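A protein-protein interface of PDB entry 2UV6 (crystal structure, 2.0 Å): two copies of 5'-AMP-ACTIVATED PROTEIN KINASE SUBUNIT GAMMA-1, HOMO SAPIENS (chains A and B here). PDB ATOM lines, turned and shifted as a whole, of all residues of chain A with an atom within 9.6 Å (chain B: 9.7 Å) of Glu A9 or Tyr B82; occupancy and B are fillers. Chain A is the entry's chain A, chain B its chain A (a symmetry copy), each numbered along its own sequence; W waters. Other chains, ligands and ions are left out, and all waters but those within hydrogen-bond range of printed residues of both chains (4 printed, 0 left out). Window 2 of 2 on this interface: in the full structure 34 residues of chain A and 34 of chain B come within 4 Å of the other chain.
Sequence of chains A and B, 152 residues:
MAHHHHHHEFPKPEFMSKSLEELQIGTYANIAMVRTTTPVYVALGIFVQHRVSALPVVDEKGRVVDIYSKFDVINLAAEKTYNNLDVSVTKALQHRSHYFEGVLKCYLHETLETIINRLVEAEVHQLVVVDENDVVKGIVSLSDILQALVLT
N of Glu A9 is in hydrogen-bond range of OH of Tyr B82. The backbone NH of Phe A10 lies within hydrogen-bond range of the backbone carbonyl oxygen of Asn B83 (2.7 Å).
The side-chain carboxylate (OE1) of Glu B79 lies within hydrogen-bond range of the side-chain amide nitrogen (ND2) of Asn B83 (3.1 Å). The backbone NH (N) of Asp B86 sits at hydrogen-bond distance from the side-chain amide oxygen (OD1) of Asn B84 (3.0 Å).
O of His A8 touches CB of Asn B84, 3.0 Å away. Leu B85 touches His A8 (N to O, 3.7 Å). Glu A9 touches Asn B83. CD2 of Leu B76 touches CD2 of Phe A10, at 3.8 Å. Phe A10 touches Ala B77. Asn B84 touches Phe A10 (CA to N, 3.7 Å). Phe A10 touches Leu B85. Ala B77 touches Pro A11 (O to CD, 3.3 Å). CG of Leu B44 touches CG1 of Val A150, at 3.8 Å.
Glu A9 touches two residues of chain B. Tyr B82 touches just one residue of chain A: Glu A9 (3.3 Å). Asn B83 touches just these residues of chain A: Glu A9 (3.4 Å) and Phe A10 (2.7 Å). Printed residues of chain B within 4 Å of His A8: Asn B84 and Leu B85. Printed residues of chain A within 4 Å of Asn B84: His A8 and Phe A10. Of the printed residues of chain A, Leu B44 touches Val A150 (3.8 Å). Glu B79 touches none of the printed residues of chain A. The nearest residue of chain B that does not touch Glu A9 is Asn B84 (4.5 Å). The nearest residue of chain A that does not touch Tyr B82 is His A8 (4.2 Å).
Of the 15 printed residues of chain B, 7 touch a printed residue of chain A. Printed residues of chain B that touch a printed residue of chain A: Leu B44, Leu B76, Ala B77, Tyr B82, Asn B83, Asn B84 and Leu B85. Of the 12 printed residues of chain A, 5 touch a printed residue of chain B.
No position is printed for both chains.
Water W2 lies within hydrogen-bond range of the side-chain hydroxyl of Tyr B82 (2.6 Å), a ring nitrogen (NE2) of His A8 (3.0 Å) and the side-chain amide nitrogen of Asn B84 (3.1 Å). Water W3 lies within hydrogen-bond range of O of Leu B76 (2.7 Å), O of Phe A10 (2.7 Å) and ND2 of Asn B83 (2.8 Å). Water W4 lies within hydrogen-bond range of the side-chain carboxylate (OE1) of Glu A9, the backbone carbonyl oxygen (O) of Phe A10 and the backbone NH (N) of Asn B83. Water W1 lies within hydrogen-bond range of NZ of Lys B80 and OE1 of Glu A113.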
ATOM      1  N   HIS A   8      16.164  14.724   1.450  1.00  0.00           N
ATOM      2  CA  HIS A   8      16.190  16.007   0.700  1.00  0.00           C
ATOM      3  C   HIS A   8      14.962  16.091  -0.205  1.00  0.00           C
ATOM      4  O   HIS A   8      14.899  16.898  -1.119  1.00  0.00           O
ATOM      5  CB  HIS A   8      17.474  16.107  -0.116  1.00  0.00           C
ATOM      6  CG  HIS A   8      17.533  15.164  -1.271  1.00  0.00           C
ATOM      7  ND1 HIS A   8      18.207  15.460  -2.443  1.00  0.00           N
ATOM      8  CD2 HIS A   8      16.996  13.935  -1.441  1.00  0.00           C
ATOM      9  CE1 HIS A   8      18.093  14.444  -3.278  1.00  0.00           C
ATOM     10  NE2 HIS A   8      17.361  13.507  -2.697  1.00  0.00           N
ATOM     11  N   GLU A   9      13.729  15.493   1.196  1.00  0.00           N
ATOM     12  CA  GLU A   9      12.433  15.868   0.713  1.00  0.00           C
ATOM     13  C   GLU A   9      12.316  17.384   0.590  1.00  0.00           C
ATOM     14  O   GLU A   9      12.833  18.122   1.438  1.00  0.00           O
ATOM     15  CB  GLU A   9      11.377  15.320   1.663  1.00  0.00           C
ATOM     16  CG  GLU A   9      10.009  15.390   1.086  1.00  0.00           C
ATOM     17  CD  GLU A   9       8.940  14.828   1.987  1.00  0.00           C
ATOM     18  OE1 GLU A   9       7.756  15.036   1.658  1.00  0.00           O
ATOM     19  OE2 GLU A   9       9.276  14.186   2.999  1.00  0.00           O
ATOM     20  N   PHE A  10      11.667  17.844  -0.481  1.00  0.00           N
ATOM     21  CA  PHE A  10      11.251  19.236  -0.589  1.00  0.00           C
ATOM     22  C   PHE A  10       9.719  19.345  -0.491  1.00  0.00           C
ATOM     23  O   PHE A  10       8.998  18.689  -1.231  1.00  0.00           O
ATOM     24  CB  PHE A  10      11.719  19.904  -1.878  1.00  0.00           C
ATOM     25  CG  PHE A  10      11.357  21.357  -1.926  1.00  0.00           C
ATOM     26  CD1 PHE A  10      12.078  22.292  -1.162  1.00  0.00           C
ATOM     27  CD2 PHE A  10      10.253  21.788  -2.638  1.00  0.00           C
ATOM     28  CE1 PHE A  10      11.713  23.638  -1.163  1.00  0.00           C
ATOM     29  CE2 PHE A  10       9.865  23.110  -2.628  1.00  0.00           C
ATOM     30  CZ  PHE A  10      10.605  24.050  -1.902  1.00  0.00           C
ATOM     31  N   PRO A  11       9.214  20.138   0.459  1.00  0.00           N
ATOM     32  CA  PRO A  11       9.892  20.865   1.508  1.00  0.00           C
ATOM     33  C   PRO A  11      10.280  19.911   2.665  1.00  0.00           C
ATOM     34  O   PRO A  11       9.714  18.808   2.771  1.00  0.00           O
ATOM     35  CB  PRO A  11       8.854  21.901   1.918  1.00  0.00           C
ATOM     36  CG  PRO A  11       7.564  21.256   1.662  1.00  0.00           C
ATOM     37  CD  PRO A  11       7.759  20.305   0.527  1.00  0.00           C
ATOM     38  N   LYS A  12      11.247  20.299   3.500  1.00  0.00           N
ATOM     39  CA  LYS A  12      11.632  19.463   4.652  1.00  0.00           C
ATOM     40  C   LYS A  12      10.459  19.349   5.611  1.00  0.00           C
ATOM     41  O   LYS A  12       9.892  20.360   6.004  1.00  0.00           O
ATOM     42  CB  LYS A  12      12.819  20.062   5.416  1.00  0.00           C
ATOM     43  CG  LYS A  12      14.121  20.117   4.640  1.00  0.00           C
ATOM     44  CD  LYS A  12      15.267  20.664   5.513  1.00  0.00           C
ATOM     45  CE  LYS A  12      16.559  19.892   5.286  1.00  0.00           C
ATOM     46  NZ  LYS A  12      16.510  18.516   5.865  1.00  0.00           N
ATOM     47  N   PRO A  13      10.078  18.124   5.989  1.00  0.00           N
ATOM     48  CA  PRO A  13       8.936  17.989   6.885  1.00  0.00           C
ATOM     49  C   PRO A  13       9.087  18.655   8.258  1.00  0.00           C
ATOM     50  O   PRO A  13       8.101  19.135   8.813  1.00  0.00           O
ATOM     51  CB  PRO A  13       8.806  16.471   7.052  1.00  0.00           C
ATOM     52  CG  PRO A  13       9.463  15.912   5.834  1.00  0.00           C
ATOM     53  CD  PRO A  13      10.623  16.812   5.608  1.00  0.00           C
ATOM     54  N   GLU A  14      10.308  18.658   8.785  1.00  0.00           N
ATOM     55  CA  GLU A  14      10.614  19.245  10.082  1.00  0.00           C
ATOM     56  C   GLU A  14      10.401  20.759  10.111  1.00  0.00           C
ATOM     57  O   GLU A  14      10.087  21.331  11.165  1.00  0.00           O
ATOM     58  CB  GLU A  14      12.044  18.861  10.551  1.00  0.00           C
ATOM     59  CG  GLU A  14      13.214  19.266   9.634  1.00  0.00           C
ATOM     60  CD  GLU A  14      13.672  18.161   8.655  1.00  0.00           C
ATOM     61  OE1 GLU A  14      14.868  18.185   8.265  1.00  0.00           O
ATOM     62  OE2 GLU A  14      12.849  17.292   8.259  1.00  0.00           O
ATOM     63  N   PHE A  15      10.505  21.396   8.949  1.00  0.00           N
ATOM     64  CA  PHE A  15      10.222  22.822   8.838  1.00  0.00           C
ATOM     65  C   PHE A  15       8.757  23.142   8.460  1.00  0.00           C
ATOM     66  O   PHE A  15       8.265  24.209   8.813  1.00  0.00           O
ATOM     67  CB  PHE A  15      11.248  23.472   7.926  1.00  0.00           C
ATOM     68  CG  PHE A  15      12.639  23.505   8.535  1.00  0.00           C
ATOM     69  CD1 PHE A  15      13.603  22.573   8.167  1.00  0.00           C
ATOM     70  CD2 PHE A  15      12.963  24.452   9.505  1.00  0.00           C
ATOM     71  CE1 PHE A  15      14.868  22.595   8.735  1.00  0.00           C
ATOM     72  CE2 PHE A  15      14.220  24.486  10.079  1.00  0.00           C
ATOM     73  CZ  PHE A  15      15.178  23.556   9.694  1.00  0.00           C
ATOM     74  N   MET A  16       8.055  22.206   7.809  1.00  0.00           N
ATOM     75  CA  MET A  16       6.606  22.348   7.552  1.00  0.00           C
ATOM     76  C   MET A  16       5.760  22.298   8.832  1.00  0.00           C
ATOM     77  O   MET A  16       4.670  22.858   8.882  1.00  0.00           O
ATOM     78  CB  MET A  16       6.116  21.251   6.599  1.00  0.00           C
ATOM     79  CG  MET A  16       6.676  21.383   5.190  1.00  0.00           C
ATOM     80  SD  MET A  16       6.031  22.849   4.351  1.00  0.00           S
ATOM     81  CE  MET A  16       4.588  22.093   3.562  1.00  0.00           C
ATOM     82  N   GLU A 113       3.232  24.562   6.812  1.00  0.00           N
ATOM     83  CA  GLU A 113       2.368  23.746   5.971  1.00  0.00           C
ATOM     84  C   GLU A 113       0.980  24.353   5.794  1.00  0.00           C
ATOM     85  O   GLU A 113       0.469  24.406   4.689  1.00  0.00           O
ATOM     86  CB  GLU A 113       2.259  22.332   6.553  1.00  0.00           C
ATOM     87  CG  GLU A 113       1.184  21.477   5.956  1.00  0.00           C
ATOM     88  CD  GLU A 113       1.125  20.128   6.596  1.00  0.00           C
ATOM     89  OE1 GLU A 113       1.416  19.131   5.910  1.00  0.00           O
ATOM     90  OE2 GLU A 113       0.803  20.074   7.799  1.00  0.00           O
ATOM     91  N   LEU A 149      12.160  28.119   3.252  1.00  0.00           N
ATOM     92  CA  LEU A 149      12.290  26.872   2.490  1.00  0.00           C
ATOM     93  C   LEU A 149      13.761  26.526   2.189  1.00  0.00           C
ATOM     94  O   LEU A 149      14.047  25.417   1.731  1.00  0.00           O
ATOM     95  CB  LEU A 149      11.429  26.906   1.211  1.00  0.00           C
ATOM     96  CG  LEU A 149       9.914  26.743   1.435  1.00  0.00           C
ATOM     97  CD1 LEU A 149       9.104  26.997   0.162  1.00  0.00           C
ATOM     98  CD2 LEU A 149       9.556  25.365   2.049  1.00  0.00           C
ATOM     99  N   VAL A 150      14.684  27.454   2.459  1.00  0.00           N
ATOM    100  CA  VAL A 150      16.129  27.188   2.315  1.00  0.00           C
ATOM    101  C   VAL A 150      16.786  26.903   3.663  1.00  0.00           C
ATOM    102  O   VAL A 150      18.017  26.897   3.751  1.00  0.00           O
ATOM    103  CB  VAL A 150      16.889  28.345   1.603  1.00  0.00           C
ATOM    104  CG1 VAL A 150      16.343  28.548   0.208  1.00  0.00           C
ATOM    105  CG2 VAL A 150      16.823  29.639   2.411  1.00  0.00           C
ATOM    106  N   LEU B  44      15.529  28.251  -6.855  1.00  0.00           N
ATOM    107  CA  LEU B  44      15.342  28.642  -5.450  1.00  0.00           C
ATOM    108  C   LEU B  44      16.535  29.462  -4.956  1.00  0.00           C
ATOM    109  O   LEU B  44      16.359  30.513  -4.342  1.00  0.00           O
ATOM    110  CB  LEU B  44      15.186  27.385  -4.607  1.00  0.00           C
ATOM    111  CG  LEU B  44      14.905  27.526  -3.102  1.00  0.00           C
ATOM    112  CD1 LEU B  44      13.726  28.484  -2.800  1.00  0.00           C
ATOM    113  CD2 LEU B  44      14.675  26.131  -2.536  1.00  0.00           C
ATOM    114  N   LEU B  76       4.888  23.745  -5.786  1.00  0.00           N
ATOM    115  CA  LEU B  76       5.699  22.533  -5.634  1.00  0.00           C
ATOM    116  C   LEU B  76       5.737  22.069  -4.181  1.00  0.00           C
ATOM    117  O   LEU B  76       5.546  20.882  -3.883  1.00  0.00           O
ATOM    118  CB  LEU B  76       7.141  22.760  -6.151  1.00  0.00           C
ATOM    119  CG  LEU B  76       8.129  21.588  -6.027  1.00  0.00           C
ATOM    120  CD1 LEU B  76       7.658  20.402  -6.862  1.00  0.00           C
ATOM    121  CD2 LEU B  76       9.580  21.973  -6.368  1.00  0.00           C
ATOM    122  N   ALA B  77       5.980  23.026  -3.286  1.00  0.00           N
ATOM    123  CA  ALA B  77       6.051  22.760  -1.862  1.00  0.00           C
ATOM    124  C   ALA B  77       4.727  22.225  -1.289  1.00  0.00           C
ATOM    125  O   ALA B  77       4.759  21.389  -0.390  1.00  0.00           O
ATOM    126  CB  ALA B  77       6.540  24.026  -1.104  1.00  0.00           C
ATOM    127  N   ALA B  78       3.579  22.682  -1.800  1.00  0.00           N
ATOM    128  CA  ALA B  78       2.271  22.173  -1.365  1.00  0.00           C
ATOM    129  C   ALA B  78       1.871  20.819  -1.982  1.00  0.00           C
ATOM    130  O   ALA B  78       0.891  20.233  -1.550  1.00  0.00           O
ATOM    131  CB  ALA B  78       1.147  23.213  -1.616  1.00  0.00           C
ATOM    132  N   GLU B  79       2.601  20.314  -2.976  1.00  0.00           N
ATOM    133  CA  GLU B  79       2.239  19.030  -3.581  1.00  0.00           C
ATOM    134  C   GLU B  79       2.266  17.945  -2.517  1.00  0.00           C
ATOM    135  O   GLU B  79       3.227  17.819  -1.769  1.00  0.00           O
ATOM    136  CB  GLU B  79       3.164  18.676  -4.754  1.00  0.00           C
ATOM    137  CG  GLU B  79       2.863  19.484  -5.991  1.00  0.00           C
ATOM    138  CD  GLU B  79       3.800  19.238  -7.151  1.00  0.00           C
ATOM    139  OE1 GLU B  79       4.369  18.145  -7.229  1.00  0.00           O
ATOM    140  OE2 GLU B  79       3.946  20.151  -8.000  1.00  0.00           O
ATOM    141  N   LYS B  80       1.196  17.169  -2.443  1.00  0.00           N
ATOM    142  CA  LYS B  80       1.109  16.105  -1.445  1.00  0.00           C
ATOM    143  C   LYS B  80       1.981  14.892  -1.813  1.00  0.00           C
ATOM    144  O   LYS B  80       2.389  14.126  -0.926  1.00  0.00           O
ATOM    145  CB  LYS B  80      -0.360  15.716  -1.190  1.00  0.00           C
ATOM    146  CG  LYS B  80      -1.280  16.924  -0.895  1.00  0.00           C
ATOM    147  CD  LYS B  80      -2.107  16.746   0.369  1.00  0.00           C
ATOM    148  CE  LYS B  80      -2.831  18.039   0.759  1.00  0.00           C
ATOM    149  NZ  LYS B  80      -1.902  19.127   1.247  1.00  0.00           N
ATOM    150  N   THR B  81       2.325  14.730  -3.091  1.00  0.00           N
ATOM    151  CA  THR B  81       3.269  13.662  -3.473  1.00  0.00           C
ATOM    152  C   THR B  81       4.694  14.047  -3.061  1.00  0.00           C
ATOM    153  O   THR B  81       4.950  15.209  -2.771  1.00  0.00           O
ATOM    154  CB  THR B  81       3.241  13.379  -4.982  1.00  0.00           C
ATOM    155  OG1 THR B  81       3.299  14.616  -5.701  1.00  0.00           O
ATOM    156  CG2 THR B  81       1.980  12.621  -5.356  1.00  0.00           C
ATOM    157  N   TYR B  82       5.601  13.073  -3.052  1.00  0.00           N
ATOM    158  CA  TYR B  82       6.975  13.282  -2.587  1.00  0.00           C
ATOM    159  C   TYR B  82       7.847  13.924  -3.655  1.00  0.00           C
ATOM    160  O   TYR B  82       7.986  13.377  -4.749  1.00  0.00           O
ATOM    161  CB  TYR B  82       7.603  11.957  -2.174  1.00  0.00           C
ATOM    162  CG  TYR B  82       9.022  12.070  -1.652  1.00  0.00           C
ATOM    163  CD1 TYR B  82       9.285  12.117  -0.283  1.00  0.00           C
ATOM    164  CD2 TYR B  82      10.108  12.154  -2.531  1.00  0.00           C
ATOM    165  CE1 TYR B  82      10.613  12.218   0.204  1.00  0.00           C
ATOM    166  CE2 TYR B  82      11.424  12.268  -2.060  1.00  0.00           C
ATOM    167  CZ  TYR B  82      11.663  12.296  -0.691  1.00  0.00           C
ATOM    168  OH  TYR B  82      12.958  12.406  -0.255  1.00  0.00           O
ATOM    169  N   ASN B  83       8.460  15.067  -3.325  1.00  0.00           N
ATOM    170  CA  ASN B  83       9.394  15.694  -4.219  1.00  0.00           C
ATOM    171  C   ASN B  83      10.679  15.953  -3.480  1.00  0.00           C
ATOM    172  O   ASN B  83      10.691  16.007  -2.253  1.00  0.00           O
ATOM    173  CB  ASN B  83       8.866  17.033  -4.782  1.00  0.00           C
ATOM    174  CG  ASN B  83       7.547  16.886  -5.530  1.00  0.00           C
ATOM    175  OD1 ASN B  83       7.475  16.238  -6.568  1.00  0.00           O
ATOM    176  ND2 ASN B  83       6.531  17.558  -5.043  1.00  0.00           N
ATOM    177  N   ASN B  84      11.757  16.062  -4.247  1.00  0.00           N
ATOM    178  CA  ASN B  84      13.005  16.649  -3.770  1.00  0.00           C
ATOM    179  C   ASN B  84      13.354  17.850  -4.667  1.00  0.00           C
ATOM    180  O   ASN B  84      12.658  18.137  -5.639  1.00  0.00           O
ATOM    181  CB  ASN B  84      14.121  15.601  -3.704  1.00  0.00           C
ATOM    182  CG  ASN B  84      14.367  14.889  -5.026  1.00  0.00           C
ATOM    183  OD1 ASN B  84      14.499  15.516  -6.085  1.00  0.00           O
ATOM    184  ND2 ASN B  84      14.464  13.574  -4.961  1.00  0.00           N
ATOM    185  N   LEU B  85      14.419  18.564  -4.350  1.00  0.00           N
ATOM    186  CA  LEU B  85      14.748  19.756  -5.122  1.00  0.00           C
ATOM    187  C   LEU B  85      15.430  19.453  -6.461  1.00  0.00           C
ATOM    188  O   LEU B  85      15.667  20.378  -7.252  1.00  0.00           O
ATOM    189  CB  LEU B  85      15.590  20.719  -4.287  1.00  0.00           C
ATOM    190  CG  LEU B  85      14.784  21.672  -3.396  1.00  0.00           C
ATOM    191  CD1 LEU B  85      15.711  22.413  -2.440  1.00  0.00           C
ATOM    192  CD2 LEU B  85      13.970  22.656  -4.249  1.00  0.00           C
ATOM    193  N   ASP B  86      15.724  18.174  -6.721  1.00  0.00           N
ATOM    194  CA  ASP B  86      16.293  17.778  -7.999  1.00  0.00           C
ATOM    195  C   ASP B  86      15.237  17.611  -9.115  1.00  0.00           C
ATOM    196  O   ASP B  86      15.530  17.085 -10.171  1.00  0.00           O
ATOM    197  CB  ASP B  86      17.128  16.503  -7.844  1.00  0.00           C
ATOM    198  CG  ASP B  86      18.193  16.364  -8.929  1.00  0.00           C
ATOM    199  OD1 ASP B  86      18.452  17.328  -9.692  1.00  0.00           O
ATOM    200  OD2 ASP B  86      18.767  15.273  -9.028  1.00  0.00           O
ATOM    201  N   VAL B  87      14.015  18.070  -8.887  1.00  0.00           N
ATOM    202  CA  VAL B  87      12.990  18.074  -9.941  1.00  0.00           C
ATOM    203  C   VAL B  87      13.343  19.237 -10.895  1.00  0.00           C
ATOM    204  O   VAL B  87      13.904  20.233 -10.443  1.00  0.00           O
ATOM    205  CB  VAL B  87      11.577  18.157  -9.285  1.00  0.00           C
ATOM    206  CG1 VAL B  87      11.309  19.536  -8.717  1.00  0.00           C
ATOM    207  CG2 VAL B  87      10.484  17.720 -10.252  1.00  0.00           C
ATOM    208  N   LYS B  91       8.582  20.753 -14.293  1.00  0.00           N
ATOM    209  CA  LYS B  91       7.454  20.113 -13.594  1.00  0.00           C
ATOM    210  C   LYS B  91       6.352  21.121 -13.217  1.00  0.00           C
ATOM    211  O   LYS B  91       5.198  20.735 -13.029  1.00  0.00           O
ATOM    212  CB  LYS B  91       7.881  19.271 -12.375  1.00  0.00           C
ATOM    213  CG  LYS B  91       6.991  17.994 -12.260  1.00  0.00           C
ATOM    214  CD  LYS B  91       7.345  17.054 -11.134  1.00  0.00           C
ATOM    215  CE  LYS B  91       6.865  17.541  -9.791  1.00  0.00           C
ATOM    216  NZ  LYS B  91       5.554  16.959  -9.462  1.00  0.00           N
ATOM    217  N   GLN B  94       2.913  21.168 -15.066  1.00  0.00           N
ATOM    218  CA  GLN B  94       1.757  20.307 -14.792  1.00  0.00           C
ATOM    219  C   GLN B  94       0.573  21.115 -14.263  1.00  0.00           C
ATOM    220  O   GLN B  94      -0.575  20.708 -14.410  1.00  0.00           O
ATOM    221  CB  GLN B  94       2.128  19.200 -13.821  1.00  0.00           C
ATOM    222  CG  GLN B  94       2.056  19.576 -12.314  1.00  0.00           C
ATOM    223  CD  GLN B  94       2.491  18.426 -11.420  1.00  0.00           C
ATOM    224  OE1 GLN B  94       3.402  17.651 -11.765  1.00  0.00           O
ATOM    225  NE2 GLN B  94       1.821  18.293 -10.262  1.00  0.00           N
HETATM  226  O   HOH W   1      -1.127  19.432   3.928  1.00  0.00           O
HETATM  227  O   HOH W   2      14.751  12.240  -2.162  1.00  0.00           O
HETATM  228  O   HOH W   3       6.657  18.851  -2.535  1.00  0.00           O
HETATM  229  O   HOH W   4       7.679  16.310  -0.757  1.00  0.00           O
